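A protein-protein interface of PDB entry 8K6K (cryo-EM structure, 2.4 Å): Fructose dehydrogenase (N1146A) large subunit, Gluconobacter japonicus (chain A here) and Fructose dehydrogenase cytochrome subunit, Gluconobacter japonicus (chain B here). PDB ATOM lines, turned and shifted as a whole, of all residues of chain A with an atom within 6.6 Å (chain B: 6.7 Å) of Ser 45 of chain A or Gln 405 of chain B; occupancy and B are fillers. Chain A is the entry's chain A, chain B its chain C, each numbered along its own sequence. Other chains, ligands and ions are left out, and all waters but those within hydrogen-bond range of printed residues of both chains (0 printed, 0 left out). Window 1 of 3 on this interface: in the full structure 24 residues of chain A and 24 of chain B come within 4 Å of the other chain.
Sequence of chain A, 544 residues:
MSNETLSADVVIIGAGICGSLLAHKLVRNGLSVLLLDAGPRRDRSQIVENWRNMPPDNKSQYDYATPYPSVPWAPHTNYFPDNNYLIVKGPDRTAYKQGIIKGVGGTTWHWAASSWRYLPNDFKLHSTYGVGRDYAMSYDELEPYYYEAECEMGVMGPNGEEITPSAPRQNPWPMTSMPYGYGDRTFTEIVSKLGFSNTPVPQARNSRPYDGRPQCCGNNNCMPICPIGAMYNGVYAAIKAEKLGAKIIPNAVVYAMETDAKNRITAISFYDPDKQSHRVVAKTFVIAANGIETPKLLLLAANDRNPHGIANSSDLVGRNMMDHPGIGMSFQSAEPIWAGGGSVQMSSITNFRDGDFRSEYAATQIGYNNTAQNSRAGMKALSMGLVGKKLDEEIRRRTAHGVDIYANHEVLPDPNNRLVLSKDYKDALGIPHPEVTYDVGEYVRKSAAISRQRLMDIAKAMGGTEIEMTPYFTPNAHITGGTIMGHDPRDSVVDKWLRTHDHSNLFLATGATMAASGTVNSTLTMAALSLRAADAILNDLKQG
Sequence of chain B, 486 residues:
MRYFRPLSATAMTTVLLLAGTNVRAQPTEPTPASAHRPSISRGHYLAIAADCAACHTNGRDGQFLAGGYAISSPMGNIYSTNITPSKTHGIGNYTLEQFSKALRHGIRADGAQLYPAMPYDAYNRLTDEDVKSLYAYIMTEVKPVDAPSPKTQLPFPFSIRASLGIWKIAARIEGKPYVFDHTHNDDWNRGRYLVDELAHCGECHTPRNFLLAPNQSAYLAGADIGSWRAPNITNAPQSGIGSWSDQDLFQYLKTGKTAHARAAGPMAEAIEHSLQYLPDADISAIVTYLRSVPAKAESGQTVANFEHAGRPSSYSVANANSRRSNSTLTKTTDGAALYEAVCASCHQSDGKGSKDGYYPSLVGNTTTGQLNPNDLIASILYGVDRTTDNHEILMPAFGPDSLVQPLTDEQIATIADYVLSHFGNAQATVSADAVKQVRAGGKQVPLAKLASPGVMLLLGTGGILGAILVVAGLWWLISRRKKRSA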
ATOM      1  N   ARG A  42      33.357 -22.597  23.959  1.00  0.00           N
ATOM      2  CA  ARG A  42      33.037 -23.970  23.599  1.00  0.00           C
ATOM      3  C   ARG A  42      31.706 -24.010  22.869  1.00  0.00           C
ATOM      4  O   ARG A  42      30.772 -23.285  23.222  1.00  0.00           O
ATOM      5  CB  ARG A  42      32.985 -24.871  24.836  1.00  0.00           C
ATOM      6  CG  ARG A  42      34.150 -24.680  25.789  1.00  0.00           C
ATOM      7  CD  ARG A  42      34.397 -25.924  26.611  1.00  0.00           C
ATOM      8  NE  ARG A  42      35.614 -25.824  27.406  1.00  0.00           N
ATOM      9  CZ  ARG A  42      36.771 -26.384  27.079  1.00  0.00           C
ATOM     10  NH1 ARG A  42      36.909 -27.083  25.967  1.00  0.00           N
ATOM     11  NH2 ARG A  42      37.814 -26.238  27.890  1.00  0.00           N
ATOM     12  N   ASP A  43      31.626 -24.856  21.848  1.00  0.00           N
ATOM     13  CA  ASP A  43      30.405 -25.054  21.083  1.00  0.00           C
ATOM     14  C   ASP A  43      29.745 -26.350  21.527  1.00  0.00           C
ATOM     15  O   ASP A  43      30.416 -27.379  21.652  1.00  0.00           O
ATOM     16  CB  ASP A  43      30.692 -25.100  19.582  1.00  0.00           C
ATOM     17  CG  ASP A  43      30.876 -23.724  18.982  1.00  0.00           C
ATOM     18  OD1 ASP A  43      30.423 -22.738  19.599  1.00  0.00           O
ATOM     19  OD2 ASP A  43      31.470 -23.627  17.890  1.00  0.00           O
ATOM     20  N   ARG A  44      28.434 -26.296  21.763  1.00  0.00           N
ATOM     21  CA  ARG A  44      27.722 -27.470  22.255  1.00  0.00           C
ATOM     22  C   ARG A  44      27.805 -28.627  21.268  1.00  0.00           C
ATOM     23  O   ARG A  44      28.047 -29.773  21.664  1.00  0.00           O
ATOM     24  CB  ARG A  44      26.266 -27.111  22.542  1.00  0.00           C
ATOM     25  CG  ARG A  44      25.307 -28.279  22.454  1.00  0.00           C
ATOM     26  CD  ARG A  44      23.882 -27.829  22.685  1.00  0.00           C
ATOM     27  NE  ARG A  44      23.818 -26.661  23.554  1.00  0.00           N
ATOM     28  CZ  ARG A  44      23.695 -26.714  24.872  1.00  0.00           C
ATOM     29  NH1 ARG A  44      23.604 -27.867  25.511  1.00  0.00           N
ATOM     30  NH2 ARG A  44      23.666 -25.581  25.565  1.00  0.00           N
ATOM     31  N   SER A  45      27.620 -28.346  19.977  1.00  0.00           N
ATOM     32  CA  SER A  45      27.613 -29.412  18.981  1.00  0.00           C
ATOM     33  C   SER A  45      28.976 -30.080  18.867  1.00  0.00           C
ATOM     34  O   SER A  45      29.063 -31.292  18.641  1.00  0.00           O
ATOM     35  CB  SER A  45      27.168 -28.860  17.631  1.00  0.00           C
ATOM     36  OG  SER A  45      25.838 -28.385  17.702  1.00  0.00           O
ATOM     37  N   GLN A  46      30.053 -29.308  19.013  1.00  0.00           N
ATOM     38  CA  GLN A  46      31.382 -29.906  18.983  1.00  0.00           C
ATOM     39  C   GLN A  46      31.602 -30.821  20.180  1.00  0.00           C
ATOM     40  O   GLN A  46      32.212 -31.886  20.048  1.00  0.00           O
ATOM     41  CB  GLN A  46      32.453 -28.823  18.932  1.00  0.00           C
ATOM     42  CG  GLN A  46      33.849 -29.370  18.726  1.00  0.00           C
ATOM     43  CD  GLN A  46      33.937 -30.328  17.556  1.00  0.00           C
ATOM     44  OE1 GLN A  46      33.482 -30.026  16.456  1.00  0.00           O
ATOM     45  NE2 GLN A  46      34.528 -31.492  17.788  1.00  0.00           N
ATOM     46  N   ILE A  47      31.113 -30.424  21.356  1.00  0.00           N
ATOM     47  CA  ILE A  47      31.213 -31.295  22.523  1.00  0.00           C
ATOM     48  C   ILE A  47      30.392 -32.558  22.310  1.00  0.00           C
ATOM     49  O   ILE A  47      30.785 -33.652  22.729  1.00  0.00           O
ATOM     50  CB  ILE A  47      30.777 -30.547  23.795  1.00  0.00           C
ATOM     51  CG1 ILE A  47      31.532 -29.224  23.933  1.00  0.00           C
ATOM     52  CG2 ILE A  47      31.006 -31.410  25.015  1.00  0.00           C
ATOM     53  CD1 ILE A  47      33.034 -29.359  23.859  1.00  0.00           C
ATOM     54  N   VAL A  48      29.237 -32.427  21.654  1.00  0.00           N
ATOM     55  CA  VAL A  48      28.413 -33.594  21.352  1.00  0.00           C
ATOM     56  C   VAL A  48      29.163 -34.549  20.435  1.00  0.00           C
ATOM     57  O   VAL A  48      29.174 -35.767  20.648  1.00  0.00           O
ATOM     58  CB  VAL A  48      27.076 -33.156  20.730  1.00  0.00           C
ATOM     59  CG1 VAL A  48      26.290 -34.361  20.263  1.00  0.00           C
ATOM     60  CG2 VAL A  48      26.279 -32.359  21.726  1.00  0.00           C
ATOM     61  N   GLU A  49      29.799 -34.006  19.398  1.00  0.00           N
ATOM     62  CA  GLU A  49      30.574 -34.840  18.484  1.00  0.00           C
ATOM     63  C   GLU A  49      31.747 -35.495  19.199  1.00  0.00           C
ATOM     64  O   GLU A  49      32.074 -36.657  18.936  1.00  0.00           O
ATOM     65  CB  GLU A  49      31.064 -34.008  17.302  1.00  0.00           C
ATOM     66  CG  GLU A  49      31.677 -34.831  16.189  1.00  0.00           C
ATOM     67  CD  GLU A  49      32.542 -34.003  15.267  1.00  0.00           C
ATOM     68  OE1 GLU A  49      33.651 -33.617  15.683  1.00  0.00           O
ATOM     69  OE2 GLU A  49      32.111 -33.738  14.127  1.00  0.00           O
ATOM     70  N   ASN A  50      32.401 -34.758  20.099  1.00  0.00           N
ATOM     71  CA  ASN A  50      33.505 -35.324  20.865  1.00  0.00           C
ATOM     72  C   ASN A  50      33.033 -36.469  21.748  1.00  0.00           C
ATOM     73  O   ASN A  50      33.717 -37.490  21.871  1.00  0.00           O
ATOM     74  CB  ASN A  50      34.166 -34.237  21.710  1.00  0.00           C
ATOM     75  CG  ASN A  50      34.946 -33.248  20.876  1.00  0.00           C
ATOM     76  OD1 ASN A  50      35.073 -33.406  19.666  1.00  0.00           O
ATOM     77  ND2 ASN A  50      35.470 -32.216  21.522  1.00  0.00           N
ATOM     78  N   ARG A  52      30.343 -38.369  21.209  1.00  0.00           N
ATOM     79  CA  ARG A  52      29.937 -39.481  20.358  1.00  0.00           C
ATOM     80  C   ARG A  52      31.134 -40.291  19.890  1.00  0.00           C
ATOM     81  O   ARG A  52      31.033 -41.512  19.726  1.00  0.00           O
ATOM     82  CB  ARG A  52      29.150 -38.962  19.158  1.00  0.00           C
ATOM     83  CG  ARG A  52      27.728 -38.563  19.476  1.00  0.00           C
ATOM     84  CD  ARG A  52      27.187 -37.617  18.428  1.00  0.00           C
ATOM     85  NE  ARG A  52      25.761 -37.373  18.599  1.00  0.00           N
ATOM     86  CZ  ARG A  52      25.058 -36.521  17.870  1.00  0.00           C
ATOM     87  NH1 ARG A  52      25.616 -35.815  16.902  1.00  0.00           N
ATOM     88  NH2 ARG A  52      23.762 -36.366  18.123  1.00  0.00           N
ATOM     89  N   TRP A 109      28.443 -26.736  31.951  1.00  0.00           N
ATOM     90  CA  TRP A 109      28.368 -27.346  30.630  1.00  0.00           C
ATOM     91  C   TRP A 109      27.982 -28.816  30.703  1.00  0.00           C
ATOM     92  O   TRP A 109      27.298 -29.322  29.808  1.00  0.00           O
ATOM     93  CB  TRP A 109      29.711 -27.203  29.914  1.00  0.00           C
ATOM     94  CG  TRP A 109      29.776 -26.087  28.926  1.00  0.00           C
ATOM     95  CD1 TRP A 109      30.594 -25.001  28.976  1.00  0.00           C
ATOM     96  CD2 TRP A 109      29.004 -25.951  27.728  1.00  0.00           C
ATOM     97  NE1 TRP A 109      30.378 -24.193  27.891  1.00  0.00           N
ATOM     98  CE2 TRP A 109      29.405 -24.755  27.108  1.00  0.00           C
ATOM     99  CE3 TRP A 109      28.010 -26.723  27.123  1.00  0.00           C
ATOM    100  CZ2 TRP A 109      28.848 -24.313  25.913  1.00  0.00           C
ATOM    101  CZ3 TRP A 109      27.460 -26.283  25.939  1.00  0.00           C
ATOM    102  CH2 TRP A 109      27.880 -25.090  25.347  1.00  0.00           C
ATOM    103  N   ILE A 225      26.893 -33.755  28.065  1.00  0.00           N
ATOM    104  CA  ILE A 225      26.450 -32.715  27.141  1.00  0.00           C
ATOM    105  C   ILE A 225      25.054 -33.000  26.604  1.00  0.00           C
ATOM    106  O   ILE A 225      24.751 -34.116  26.172  1.00  0.00           O
ATOM    107  CB  ILE A 225      27.461 -32.533  25.989  1.00  0.00           C
ATOM    108  CG1 ILE A 225      27.034 -31.378  25.083  1.00  0.00           C
ATOM    109  CG2 ILE A 225      27.651 -33.823  25.206  1.00  0.00           C
ATOM    110  CD1 ILE A 225      27.305 -30.017  25.665  1.00  0.00           C
ATOM    111  N   CYS A 226      24.195 -31.985  26.635  1.00  0.00           N
ATOM    112  CA  CYS A 226      22.901 -32.050  25.973  1.00  0.00           C
ATOM    113  C   CYS A 226      23.071 -31.697  24.505  1.00  0.00           C
ATOM    114  O   CYS A 226      23.606 -30.625  24.198  1.00  0.00           O
ATOM    115  CB  CYS A 226      21.916 -31.096  26.617  1.00  0.00           C
ATOM    116  SG  CYS A 226      20.199 -31.355  26.133  1.00  0.00           S
ATOM    117  N   PRO A 227      22.643 -32.548  23.573  1.00  0.00           N
ATOM    118  CA  PRO A 227      22.805 -32.211  22.154  1.00  0.00           C
ATOM    119  C   PRO A 227      21.870 -31.118  21.683  1.00  0.00           C
ATOM    120  O   PRO A 227      22.138 -30.506  20.643  1.00  0.00           O
ATOM    121  CB  PRO A 227      22.515 -33.537  21.434  1.00  0.00           C
ATOM    122  CG  PRO A 227      22.246 -34.549  22.506  1.00  0.00           C
ATOM    123  CD  PRO A 227      21.938 -33.822  23.759  1.00  0.00           C
ATOM    124  N   LEU B 329      33.749 -25.713  17.328  1.00  0.00           N
ATOM    125  CA  LEU B 329      33.901 -26.185  15.956  1.00  0.00           C
ATOM    126  C   LEU B 329      34.105 -25.045  14.969  1.00  0.00           C
ATOM    127  O   LEU B 329      33.241 -24.178  14.807  1.00  0.00           O
ATOM    128  CB  LEU B 329      32.672 -27.009  15.549  1.00  0.00           C
ATOM    129  CG  LEU B 329      31.248 -26.483  15.764  1.00  0.00           C
ATOM    130  CD1 LEU B 329      30.686 -25.858  14.506  1.00  0.00           C
ATOM    131  CD2 LEU B 329      30.339 -27.602  16.212  1.00  0.00           C
ATOM    132  N   LEU B 338      28.556 -31.402  10.141  1.00  0.00           N
ATOM    133  CA  LEU B 338      27.845 -30.317  10.806  1.00  0.00           C
ATOM    134  C   LEU B 338      26.393 -30.686  11.064  1.00  0.00           C
ATOM    135  O   LEU B 338      25.860 -30.422  12.149  1.00  0.00           O
ATOM    136  CB  LEU B 338      27.932 -29.042   9.969  1.00  0.00           C
ATOM    137  CG  LEU B 338      29.201 -28.208  10.112  1.00  0.00           C
ATOM    138  CD1 LEU B 338      29.240 -27.121   9.056  1.00  0.00           C
ATOM    139  CD2 LEU B 338      29.287 -27.611  11.502  1.00  0.00           C
ATOM    140  N   GLU B 340      25.197 -33.704  11.440  1.00  0.00           N
ATOM    141  CA  GLU B 340      25.164 -34.713  12.489  1.00  0.00           C
ATOM    142  C   GLU B 340      25.378 -34.095  13.863  1.00  0.00           C
ATOM    143  O   GLU B 340      24.690 -34.450  14.826  1.00  0.00           O
ATOM    144  CB  GLU B 340      26.210 -35.791  12.222  1.00  0.00           C
ATOM    145  CG  GLU B 340      26.082 -36.984  13.142  1.00  0.00           C
ATOM    146  CD  GLU B 340      25.071 -37.990  12.644  1.00  0.00           C
ATOM    147  OE1 GLU B 340      24.567 -37.821  11.516  1.00  0.00           O
ATOM    148  OE2 GLU B 340      24.779 -38.953  13.380  1.00  0.00           O
ATOM    149  N   ALA B 341      26.328 -33.168  13.974  1.00  0.00           N
ATOM    150  CA  ALA B 341      26.623 -32.572  15.271  1.00  0.00           C
ATOM    151  C   ALA B 341      25.481 -31.690  15.754  1.00  0.00           C
ATOM    152  O   ALA B 341      25.148 -31.698  16.944  1.00  0.00           O
ATOM    153  CB  ALA B 341      27.923 -31.774  15.197  1.00  0.00           C
ATOM    154  N   VAL B 342      24.864 -30.931  14.855  1.00  0.00           N
ATOM    155  CA  VAL B 342      23.886 -29.923  15.241  1.00  0.00           C
ATOM    156  C   VAL B 342      22.459 -30.448  15.157  1.00  0.00           C
ATOM    157  O   VAL B 342      21.659 -30.211  16.062  1.00  0.00           O
ATOM    158  CB  VAL B 342      24.059 -28.653  14.380  1.00  0.00           C
ATOM    159  CG1 VAL B 342      23.135 -27.557  14.870  1.00  0.00           C
ATOM    160  CG2 VAL B 342      25.498 -28.185  14.410  1.00  0.00           C
ATOM    161  N   CYS B 343      22.117 -31.167  14.088  1.00  0.00           N
ATOM    162  CA  CYS B 343      20.726 -31.466  13.789  1.00  0.00           C
ATOM    163  C   CYS B 343      20.338 -32.930  13.925  1.00  0.00           C
ATOM    164  O   CYS B 343      19.144 -33.216  14.049  1.00  0.00           O
ATOM    165  CB  CYS B 343      20.377 -31.011  12.363  1.00  0.00           C
ATOM    166  SG  CYS B 343      21.309 -29.582  11.783  1.00  0.00           S
ATOM    167  N   PRO B 396      14.708 -25.069  18.461  1.00  0.00           N
ATOM    168  CA  PRO B 396      15.637 -24.007  18.855  1.00  0.00           C
ATOM    169  C   PRO B 396      16.160 -23.268  17.633  1.00  0.00           C
ATOM    170  O   PRO B 396      16.348 -23.850  16.564  1.00  0.00           O
ATOM    171  CB  PRO B 396      16.752 -24.765  19.581  1.00  0.00           C
ATOM    172  CG  PRO B 396      16.688 -26.143  19.025  1.00  0.00           C
ATOM    173  CD  PRO B 396      15.243 -26.410  18.743  1.00  0.00           C
ATOM    174  N   ALA B 397      16.383 -21.968  17.795  1.00  0.00           N
ATOM    175  CA  ALA B 397      17.006 -21.190  16.738  1.00  0.00           C
ATOM    176  C   ALA B 397      18.486 -21.530  16.643  1.00  0.00           C
ATOM    177  O   ALA B 397      19.120 -21.923  17.625  1.00  0.00           O
ATOM    178  CB  ALA B 397      16.823 -19.696  16.991  1.00  0.00           C
ATOM    179  N   PHE B 398      19.041 -21.384  15.437  1.00  0.00           N
ATOM    180  CA  PHE B 398      20.453 -21.664  15.211  1.00  0.00           C
ATOM    181  C   PHE B 398      21.155 -20.514  14.500  1.00  0.00           C
ATOM    182  O   PHE B 398      22.196 -20.724  13.873  1.00  0.00           O
ATOM    183  CB  PHE B 398      20.628 -22.963  14.426  1.00  0.00           C
ATOM    184  CG  PHE B 398      20.248 -24.186  15.201  1.00  0.00           C
ATOM    185  CD1 PHE B 398      21.087 -24.692  16.175  1.00  0.00           C
ATOM    186  CD2 PHE B 398      19.046 -24.825  14.965  1.00  0.00           C
ATOM    187  CE1 PHE B 398      20.736 -25.811  16.893  1.00  0.00           C
ATOM    188  CE2 PHE B 398      18.692 -25.944  15.681  1.00  0.00           C
ATOM    189  CZ  PHE B 398      19.538 -26.439  16.645  1.00  0.00           C
ATOM    190  N   GLY B 399      20.612 -19.305  14.590  1.00  0.00           N
ATOM    191  CA  GLY B 399      21.245 -18.142  14.022  1.00  0.00           C
ATOM    192  C   GLY B 399      22.290 -17.574  14.956  1.00  0.00           C
ATOM    193  O   GLY B 399      22.712 -18.223  15.917  1.00  0.00           O
ATOM    194  N   SER B 402      21.415 -17.546  18.673  1.00  0.00           N
ATOM    195  CA  SER B 402      21.009 -18.830  19.217  1.00  0.00           C
ATOM    196  C   SER B 402      21.586 -19.046  20.609  1.00  0.00           C
ATOM    197  O   SER B 402      22.704 -18.629  20.918  1.00  0.00           O
ATOM    198  CB  SER B 402      21.458 -19.961  18.297  1.00  0.00           C
ATOM    199  OG  SER B 402      21.036 -21.217  18.795  1.00  0.00           O
ATOM    200  N   LEU B 403      20.800 -19.710  21.454  1.00  0.00           N
ATOM    201  CA  LEU B 403      21.270 -20.137  22.764  1.00  0.00           C
ATOM    202  C   LEU B 403      21.834 -21.548  22.741  1.00  0.00           C
ATOM    203  O   LEU B 403      22.748 -21.857  23.513  1.00  0.00           O
ATOM    204  CB  LEU B 403      20.131 -20.068  23.783  1.00  0.00           C
ATOM    205  CG  LEU B 403      19.841 -18.715  24.429  1.00  0.00           C
ATOM    206  CD1 LEU B 403      18.835 -18.878  25.550  1.00  0.00           C
ATOM    207  CD2 LEU B 403      21.117 -18.082  24.946  1.00  0.00           C
ATOM    208  N   VAL B 404      21.312 -22.405  21.867  1.00  0.00           N
ATOM    209  CA  VAL B 404      21.737 -23.800  21.833  1.00  0.00           C
ATOM    210  C   VAL B 404      23.054 -23.945  21.081  1.00  0.00           C
ATOM    211  O   VAL B 404      24.040 -24.466  21.613  1.00  0.00           O
ATOM    212  CB  VAL B 404      20.636 -24.677  21.214  1.00  0.00           C
ATOM    213  CG1 VAL B 404      21.130 -26.095  21.023  1.00  0.00           C
ATOM    214  CG2 VAL B 404      19.398 -24.651  22.086  1.00  0.00           C
ATOM    215  N   GLN B 405      23.089 -23.485  19.838  1.00  0.00           N
ATOM    216  CA  GLN B 405      24.298 -23.578  19.033  1.00  0.00           C
ATOM    217  C   GLN B 405      24.294 -22.509  17.950  1.00  0.00           C
ATOM    218  O   GLN B 405      23.709 -22.714  16.880  1.00  0.00           O
ATOM    219  CB  GLN B 405      24.426 -24.966  18.407  1.00  0.00           C
ATOM    220  CG  GLN B 405      25.643 -25.134  17.517  1.00  0.00           C
ATOM    221  CD  GLN B 405      26.928 -24.741  18.209  1.00  0.00           C
ATOM    222  OE1 GLN B 405      27.440 -25.476  19.048  1.00  0.00           O
ATOM    223  NE2 GLN B 405      27.457 -23.577  17.860  1.00  0.00           N
ATOM    224  N   PRO B 406      24.911 -21.355  18.191  1.00  0.00           N
ATOM    225  CA  PRO B 406      25.019 -20.347  17.132  1.00  0.00           C
ATOM    226  C   PRO B 406      25.800 -20.886  15.945  1.00  0.00           C
ATOM    227  O   PRO B 406      26.808 -21.577  16.102  1.00  0.00           O
ATOM    228  CB  PRO B 406      25.757 -19.190  17.813  1.00  0.00           C
ATOM    229  CG  PRO B 406      25.603 -19.432  19.273  1.00  0.00           C
ATOM    230  CD  PRO B 406      25.524 -20.907  19.450  1.00  0.00           C
ATOM    231  N   LEU B 407      25.331 -20.554  14.749  1.00  0.00           N
ATOM    232  CA  LEU B 407      25.973 -20.982  13.517  1.00  0.00           C
ATOM    233  C   LEU B 407      26.240 -19.771  12.641  1.00  0.00           C
ATOM    234  O   LEU B 407      25.434 -18.840  12.590  1.00  0.00           O
ATOM    235  CB  LEU B 407      25.114 -21.993  12.754  1.00  0.00           C
ATOM    236  CG  LEU B 407      24.787 -23.316  13.445  1.00  0.00           C
ATOM    237  CD1 LEU B 407      23.816 -24.116  12.602  1.00  0.00           C
ATOM    238  CD2 LEU B 407      26.051 -24.110  13.706  1.00  0.00           C
ATOM    239  N   GLN B 411      28.331 -21.939   7.903  1.00  0.00           N
ATOM    240  CA  GLN B 411      27.901 -23.200   8.502  1.00  0.00           C
ATOM    241  C   GLN B 411      26.445 -23.502   8.174  1.00  0.00           C
ATOM    242  O   GLN B 411      26.100 -24.644   7.843  1.00  0.00           O
ATOM    243  CB  GLN B 411      28.109 -23.160  10.014  1.00  0.00           C
ATOM    244  CG  GLN B 411      29.540 -23.399  10.445  1.00  0.00           C
ATOM    245  CD  GLN B 411      29.815 -22.898  11.842  1.00  0.00           C
ATOM    246  OE1 GLN B 411      29.014 -22.169  12.422  1.00  0.00           O
ATOM    247  NE2 GLN B 411      30.957 -23.283  12.392  1.00  0.00           N
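Gln 405 of chain B touches Asp 43 of chain A. Leu 329 of chain B touches Ser 45 of chain A. Ser 45 of chain A touches Val 342 of chain B. Gln 46 of chain A touches Leu 329 of chain B (OE1 to CB, 3.3 Å). CA of Ala 341 of chain B touches NH1 of Arg 52 of chain A, 3.8 Å away.
Of the printed residues of chain B, Ser 45 of chain A touches Leu 329, Ala 341, Val 342 and Gln 405. Of chain A, only Asp 43 (3.3 Å), Arg 44 (3.0 Å) and Ser 45 (3.0 Å) come within 4 Å of Gln 405 of chain B. Of the printed residues of chain A, Val 342 of chain B touches Ser 45. Of the printed residues of chain B, Asp 43 of chain A touches Leu 329 (3.1 Å) and Gln 405 (3.3 Å). Printed residues of chain B within 4 Å of Arg 44 of chain A: Val 404 (2.9 Å) and Gln 405 (3.0 Å). Val 48 of chain A touches none of the printed residues of chain B. The nearest residue of chain B that does not touch Ser 45 of chain A is Val 404 of chain B (5.5 Å). The nearest residue of chain A that does not touch Gln 405 of chain B is Gln 46 of chain A (4.6 Å). The nearest printed residue of chain A that does not touch Val 404 of chain B is Pro 227 of chain A (4.5 Å).
O of Cys 226 of chain A lies within hydrogen-bond range of NH1 of Arg 44 of chain A, at 3.1 Å. The side-chain amide nitrogen of Gln 46 of chain A is in hydrogen-bond range of the side-chain carboxylate of Glu 49 of chain A (3.1 Å). The side-chain amide oxygen (OD1) of Asn 50 of chain A sits at hydrogen-bond distance from the side-chain amide nitrogen (NE2) of Gln 46 of chain A (2.7 Å). NE2 of Gln 411 of chain B sits close to O of Leu 329 of chain B (3.4 Å). The side-chain hydroxyl (OG) of Ser 402 of chain B is in hydrogen-bond range of the backbone NH (N) of Val 404 of chain B. The side-chain hydroxyl (OG) of Ser 402 of chain B lies within hydrogen-bond range of the backbone NH (N) of Gln 405 of chain B, at 3.2 Å.
Along chain A the printed residues that touch a printed residue of chain B span positions 43 to 52. Of the 17 printed residues of chain B, 6 touch a printed residue of chain A. Printed residues of chain B that touch a printed residue of chain A: Leu 329, Glu 340, Ala 341, Val 342, Val 404 and Gln 405. Hydrophobic or aromatic side chains of chain B that line the printed part of chain A: Leu 329, Ala 341, Val 342 and Val 404. Along chain B the printed residues that touch a printed residue of chain A span positions 329 to 405.
The side-chain carboxylate of Asp 43 of chain A sits at hydrogen-bond distance from the backbone NH of Leu 329 of chain B (3.1 Å). The backbone carbonyl oxygen of Val 404 of chain B is in hydrogen-bond range of the guanidinium group of Arg 44 of chain A (2.9 Å). The backbone NH (N) of Arg 44 of chain A lies within hydrogen-bond range of the side-chain amide oxygen (OE1) of Gln 405 of chain B. OG of Ser 45 of chain A sits at hydrogen-bond distance from O of Ala 341 of chain B, at 3.5 Å. The side-chain amide oxygen (OE1) of Gln 405 of chain B is in hydrogen-bond range of the backbone NH (N) of Ser 45 of chain A (3.0 Å). The guanidinium group (NH1) of Arg 52 of chain A lies within hydrogen-bond range of the backbone carbonyl oxygen (O) of Glu 340 of chain B.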
